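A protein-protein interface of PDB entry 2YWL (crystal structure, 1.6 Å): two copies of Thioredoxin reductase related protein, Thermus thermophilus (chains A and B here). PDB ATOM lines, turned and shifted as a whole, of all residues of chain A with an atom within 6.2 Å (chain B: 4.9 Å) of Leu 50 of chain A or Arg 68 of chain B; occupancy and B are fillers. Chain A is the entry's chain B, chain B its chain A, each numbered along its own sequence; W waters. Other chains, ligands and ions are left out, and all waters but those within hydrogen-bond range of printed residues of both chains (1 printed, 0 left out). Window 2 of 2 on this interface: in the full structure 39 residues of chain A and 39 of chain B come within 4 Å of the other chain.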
ATOM      1  N   PRO A  44       3.039  21.103  -9.180  1.00  0.00           N
ATOM      2  CA  PRO A  44       3.093  22.264  -8.292  1.00  0.00           C
ATOM      3  C   PRO A  44       4.465  22.648  -7.777  1.00  0.00           C
ATOM      4  O   PRO A  44       4.594  23.625  -7.038  1.00  0.00           O
ATOM      5  CB  PRO A  44       2.184  21.837  -7.154  1.00  0.00           C
ATOM      6  CG  PRO A  44       2.600  20.402  -6.977  1.00  0.00           C
ATOM      7  CD  PRO A  44       2.735  19.879  -8.412  1.00  0.00           C
ATOM      8  N   TYR A  46       7.695  22.994  -9.774  1.00  0.00           N
ATOM      9  CA  TYR A  46       8.754  23.265 -10.742  1.00  0.00           C
ATOM     10  C   TYR A  46       8.959  24.762 -10.511  1.00  0.00           C
ATOM     11  O   TYR A  46       8.226  25.594 -11.048  1.00  0.00           O
ATOM     12  CB  TYR A  46       8.291  22.991 -12.177  1.00  0.00           C
ATOM     13  CG  TYR A  46       9.420  22.978 -13.189  1.00  0.00           C
ATOM     14  CD1 TYR A  46      10.129  21.807 -13.464  1.00  0.00           C
ATOM     15  CD2 TYR A  46       9.787  24.143 -13.867  1.00  0.00           C
ATOM     16  CE1 TYR A  46      11.176  21.795 -14.397  1.00  0.00           C
ATOM     17  CE2 TYR A  46      10.830  24.141 -14.800  1.00  0.00           C
ATOM     18  CZ  TYR A  46      11.516  22.963 -15.061  1.00  0.00           C
ATOM     19  OH  TYR A  46      12.523  22.958 -16.003  1.00  0.00           O
ATOM     20  N   PRO A  47       9.954  25.121  -9.685  1.00  0.00           N
ATOM     21  CA  PRO A  47      10.276  26.510  -9.340  1.00  0.00           C
ATOM     22  C   PRO A  47      10.147  27.538 -10.454  1.00  0.00           C
ATOM     23  O   PRO A  47      10.898  27.515 -11.427  1.00  0.00           O
ATOM     24  CB  PRO A  47      11.698  26.409  -8.804  1.00  0.00           C
ATOM     25  CG  PRO A  47      11.708  25.051  -8.161  1.00  0.00           C
ATOM     26  CD  PRO A  47      11.000  24.206  -9.189  1.00  0.00           C
ATOM     27  N   GLY A  48       9.186  28.445 -10.300  1.00  0.00           N
ATOM     28  CA  GLY A  48       8.994  29.479 -11.299  1.00  0.00           C
ATOM     29  C   GLY A  48       7.736  29.357 -12.139  1.00  0.00           C
ATOM     30  O   GLY A  48       7.191  30.367 -12.580  1.00  0.00           O
ATOM     31  N   LEU A  49       7.278  28.132 -12.383  1.00  0.00           N
ATOM     32  CA  LEU A  49       6.068  27.931 -13.177  1.00  0.00           C
ATOM     33  C   LEU A  49       4.854  28.009 -12.259  1.00  0.00           C
ATOM     34  O   LEU A  49       4.317  26.989 -11.826  1.00  0.00           O
ATOM     35  CB  LEU A  49       6.109  26.577 -13.892  1.00  0.00           C
ATOM     36  CG  LEU A  49       6.909  26.520 -15.197  1.00  0.00           C
ATOM     37  CD1 LEU A  49       8.348  26.915 -14.939  1.00  0.00           C
ATOM     38  CD2 LEU A  49       6.839  25.123 -15.782  1.00  0.00           C
ATOM     39  N   LEU A  50       4.436  29.238 -11.976  1.00  0.00           N
ATOM     40  CA  LEU A  50       3.312  29.514 -11.089  1.00  0.00           C
ATOM     41  C   LEU A  50       1.963  28.983 -11.555  1.00  0.00           C
ATOM     42  O   LEU A  50       1.049  28.817 -10.746  1.00  0.00           O
ATOM     43  CB  LEU A  50       3.198  31.023 -10.855  1.00  0.00           C
ATOM     44  CG  LEU A  50       4.394  31.703 -10.187  1.00  0.00           C
ATOM     45  CD1 LEU A  50       4.174  33.211 -10.173  1.00  0.00           C
ATOM     46  CD2 LEU A  50       4.568  31.166  -8.774  1.00  0.00           C
ATOM     47  N   ASP A  51       1.831  28.721 -12.850  1.00  0.00           N
ATOM     48  CA  ASP A  51       0.567  28.213 -13.369  1.00  0.00           C
ATOM     49  C   ASP A  51       0.414  26.714 -13.114  1.00  0.00           C
ATOM     50  O   ASP A  51      -0.625  26.129 -13.414  1.00  0.00           O
ATOM     51  CB  ASP A  51       0.453  28.513 -14.866  1.00  0.00           C
ATOM     52  CG  ASP A  51       1.490  27.779 -15.688  1.00  0.00           C
ATOM     53  OD1 ASP A  51       2.692  27.892 -15.373  1.00  0.00           O
ATOM     54  OD2 ASP A  51       1.097  27.092 -16.653  1.00  0.00           O
ATOM     55  N   GLU A  52       1.457  26.104 -12.554  1.00  0.00           N
ATOM     56  CA  GLU A  52       1.472  24.677 -12.228  1.00  0.00           C
ATOM     57  C   GLU A  52       0.797  23.827 -13.305  1.00  0.00           C
ATOM     58  O   GLU A  52      -0.232  23.194 -13.065  1.00  0.00           O
ATOM     59  CB  GLU A  52       0.802  24.454 -10.866  1.00  0.00           C
ATOM     60  CG  GLU A  52       1.257  25.460  -9.812  1.00  0.00           C
ATOM     61  CD  GLU A  52       0.821  25.103  -8.400  1.00  0.00           C
ATOM     62  OE1 GLU A  52      -0.188  24.388  -8.241  1.00  0.00           O
ATOM     63  OE2 GLU A  52       1.487  25.556  -7.445  1.00  0.00           O
ATOM     64  N   PRO A  53       1.385  23.796 -14.509  1.00  0.00           N
ATOM     65  CA  PRO A  53       0.851  23.029 -15.637  1.00  0.00           C
ATOM     66  C   PRO A  53       0.910  21.521 -15.431  1.00  0.00           C
ATOM     67  O   PRO A  53       1.631  21.026 -14.565  1.00  0.00           O
ATOM     68  CB  PRO A  53       1.728  23.483 -16.798  1.00  0.00           C
ATOM     69  CG  PRO A  53       3.049  23.688 -16.135  1.00  0.00           C
ATOM     70  CD  PRO A  53       2.656  24.444 -14.878  1.00  0.00           C
ATOM     71  N   ARG B  61       9.243  35.452  -9.309  1.00  0.00           N
ATOM     72  CA  ARG B  61       8.370  34.292  -9.468  1.00  0.00           C
ATOM     73  C   ARG B  61       8.774  33.171  -8.519  1.00  0.00           C
ATOM     74  O   ARG B  61       7.917  32.508  -7.937  1.00  0.00           O
ATOM     75  CB  ARG B  61       8.402  33.787 -10.914  1.00  0.00           C
ATOM     76  CG  ARG B  61       7.833  34.781 -11.913  1.00  0.00           C
ATOM     77  CD  ARG B  61       7.935  34.267 -13.338  1.00  0.00           C
ATOM     78  NE  ARG B  61       7.516  35.279 -14.303  1.00  0.00           N
ATOM     79  CZ  ARG B  61       7.565  35.119 -15.621  1.00  0.00           C
ATOM     80  NH1 ARG B  61       8.012  33.983 -16.140  1.00  0.00           N
ATOM     81  NH2 ARG B  61       7.168  36.100 -16.420  1.00  0.00           N
ATOM     82  N   ALA B  64       7.553  34.064  -5.091  1.00  0.00           N
ATOM     83  CA  ALA B  64       6.104  33.925  -5.015  1.00  0.00           C
ATOM     84  C   ALA B  64       5.719  32.457  -4.904  1.00  0.00           C
ATOM     85  O   ALA B  64       4.807  32.096  -4.161  1.00  0.00           O
ATOM     86  CB  ALA B  64       5.450  34.545  -6.246  1.00  0.00           C
ATOM     87  N   HIS B  65       6.430  31.613  -5.642  1.00  0.00           N
ATOM     88  CA  HIS B  65       6.161  30.184  -5.639  1.00  0.00           C
ATOM     89  C   HIS B  65       6.428  29.587  -4.255  1.00  0.00           C
ATOM     90  O   HIS B  65       5.640  28.790  -3.752  1.00  0.00           O
ATOM     91  CB  HIS B  65       7.031  29.501  -6.700  1.00  0.00           C
ATOM     92  CG  HIS B  65       6.460  28.216  -7.215  1.00  0.00           C
ATOM     93  ND1 HIS B  65       6.914  27.612  -8.368  1.00  0.00           N
ATOM     94  CD2 HIS B  65       5.480  27.416  -6.732  1.00  0.00           C
ATOM     95  CE1 HIS B  65       6.238  26.495  -8.573  1.00  0.00           C
ATOM     96  NE2 HIS B  65       5.362  26.353  -7.595  1.00  0.00           N
ATOM     97  N   ALA B  66       7.533  29.984  -3.636  1.00  0.00           N
ATOM     98  CA  ALA B  66       7.884  29.473  -2.314  1.00  0.00           C
ATOM     99  C   ALA B  66       6.883  29.940  -1.261  1.00  0.00           C
ATOM    100  O   ALA B  66       6.480  29.166  -0.388  1.00  0.00           O
ATOM    101  CB  ALA B  66       9.297  29.917  -1.938  1.00  0.00           C
ATOM    102  N   ARG B  67       6.481  31.206  -1.342  1.00  0.00           N
ATOM    103  CA  ARG B  67       5.519  31.758  -0.393  1.00  0.00           C
ATOM    104  C   ARG B  67       4.165  31.073  -0.511  1.00  0.00           C
ATOM    105  O   ARG B  67       3.458  30.908   0.487  1.00  0.00           O
ATOM    106  CB  ARG B  67       5.345  33.262  -0.619  1.00  0.00           C
ATOM    107  CG  ARG B  67       6.523  34.106  -0.171  1.00  0.00           C
ATOM    108  CD  ARG B  67       6.234  35.579  -0.408  1.00  0.00           C
ATOM    109  NE  ARG B  67       7.323  36.441   0.039  1.00  0.00           N
ATOM    110  CZ  ARG B  67       7.634  36.662   1.311  1.00  0.00           C
ATOM    111  NH1 ARG B  67       6.937  36.084   2.281  1.00  0.00           N
ATOM    112  NH2 ARG B  67       8.646  37.466   1.613  1.00  0.00           N
ATOM    113  N   ARG B  68       3.804  30.680  -1.729  1.00  0.00           N
ATOM    114  CA  ARG B  68       2.529  30.011  -1.968  1.00  0.00           C
ATOM    115  C   ARG B  68       2.364  28.791  -1.079  1.00  0.00           C
ATOM    116  O   ARG B  68       1.246  28.437  -0.690  1.00  0.00           O
ATOM    117  CB  ARG B  68       2.418  29.579  -3.434  1.00  0.00           C
ATOM    118  CG  ARG B  68       1.227  28.674  -3.724  1.00  0.00           C
ATOM    119  CD  ARG B  68       1.124  28.378  -5.206  1.00  0.00           C
ATOM    120  NE  ARG B  68       0.827  29.586  -5.971  1.00  0.00           N
ATOM    121  CZ  ARG B  68       0.855  29.657  -7.298  1.00  0.00           C
ATOM    122  NH1 ARG B  68       1.171  28.587  -8.012  1.00  0.00           N
ATOM    123  NH2 ARG B  68       0.561  30.798  -7.909  1.00  0.00           N
ATOM    124  N   TYR B  69       3.474  28.144  -0.745  1.00  0.00           N
ATOM    125  CA  TYR B  69       3.396  26.957   0.084  1.00  0.00           C
ATOM    126  C   TYR B  69       3.920  27.101   1.510  1.00  0.00           C
ATOM    127  O   TYR B  69       4.177  26.107   2.185  1.00  0.00           O
ATOM    128  CB  TYR B  69       4.047  25.783  -0.658  1.00  0.00           C
ATOM    129  CG  TYR B  69       3.231  25.407  -1.880  1.00  0.00           C
ATOM    130  CD1 TYR B  69       1.963  24.844  -1.739  1.00  0.00           C
ATOM    131  CD2 TYR B  69       3.679  25.699  -3.172  1.00  0.00           C
ATOM    132  CE1 TYR B  69       1.153  24.588  -2.846  1.00  0.00           C
ATOM    133  CE2 TYR B  69       2.874  25.445  -4.290  1.00  0.00           C
ATOM    134  CZ  TYR B  69       1.613  24.893  -4.116  1.00  0.00           C
ATOM    135  OH  TYR B  69       0.793  24.665  -5.202  1.00  0.00           O
ATOM    136  N   GLY B  70       4.070  28.343   1.964  1.00  0.00           N
ATOM    137  CA  GLY B  70       4.486  28.564   3.339  1.00  0.00           C
ATOM    138  C   GLY B  70       5.842  29.136   3.687  1.00  0.00           C
ATOM    139  O   GLY B  70       6.060  29.513   4.840  1.00  0.00           O
HETATM  140  O   HOH W   1       6.547  31.465 -15.015  1.00  0.00           O
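No position is printed for both chains. Of the 13 pairs that touch across the chains among the printed residues, none has its exchanged pair printed and touching as well.
Of the 9 printed residues of chain A, 7 touch a printed residue of chain B. Printed residues of chain A that touch a printed residue of chain B: Pro 44, Tyr 46, Pro 47, Gly 48, Leu 49, Leu 50 and Glu 52. Printed residues of chain B that touch a printed residue of chain A: Arg 61, His 65, Arg 68 and Tyr 69. Hydrophobic or aromatic side chains of chain B that line the printed part of chain A: His 65 and Tyr 69.
Water W1 lies within hydrogen-bond range of the backbone carbonyl oxygen (O) of Gly 48 of chain A and the guanidinium group (NH1) of Arg 61 of chain B.
NE2 of His 65 of chain B is in hydrogen-bond range of O of Pro 44 of chain A. A ring nitrogen (ND1) of His 65 of chain B lies within hydrogen-bond range of the backbone NH of Gly 48 of chain A. The guanidinium group of Arg 68 of chain B lies within hydrogen-bond range of the backbone carbonyl oxygen of Leu 50 of chain A (2.7 Å). The side-chain carboxylate (OE2) of Glu 52 of chain A is in salt-bridge range of the guanidinium group (NH1) of Arg 68 of chain B (3.1 Å). OH of Tyr 69 of chain B is in hydrogen-bond range of OE2 of Glu 52 of chain A (2.5 Å).
Of the printed residues of chain B, Tyr 46 of chain A touches His 65 (3.3 Å). Of the printed residues of chain B, Gly 48 of chain A touches Arg 61 (3.99 Å) and His 65 (3.1 Å). Of chain B, only Arg 61, His 65 and Arg 68 come within 4 Å of Leu 50 of chain A. Asp 51 of chain A touches none of the printed residues of chain B. Of the printed residues of chain B, Glu 52 of chain A touches His 65, Arg 68 and Tyr 69. Of the printed residues of chain A, His 65 of chain B touches Pro 44 (2.9 Å), Tyr 46 (3.3 Å), Pro 47 (3.7 Å), Gly 48 (3.1 Å), Leu 49 (3.8 Å), Leu 50 (3.6 Å) and Glu 52 (3.96 Å). Ala 66 of chain B touches none of the printed residues of chain A. Of the printed residues of chain A, Arg 68 of chain B touches Leu 50 (2.7 Å) and Glu 52 (3.1 Å). The nearest printed residue of chain B that does not touch Pro 44 of chain A is Arg 68 of chain B (6.1 Å).
Among the printed residues, merely in contact across the chains: Pro 44 of chain A with Tyr 69 of chain B (3.7 Å), Tyr 46 of chain A with His 65 of chain B (3.3 Å), Pro 47 of chain A with His 65 of chain B (3.7 Å), Gly 48 of chain A with Arg 61 of chain B (3.99 Å), Leu 49 of chain A with His 65 of chain B (3.8 Å), Leu 50 of chain A with Arg 61 of chain B (3.7 Å), Leu 50 of chain A with His 65 of chain B (3.6 Å) and Glu 52 of chain A with His 65 of chain B (3.96 Å).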
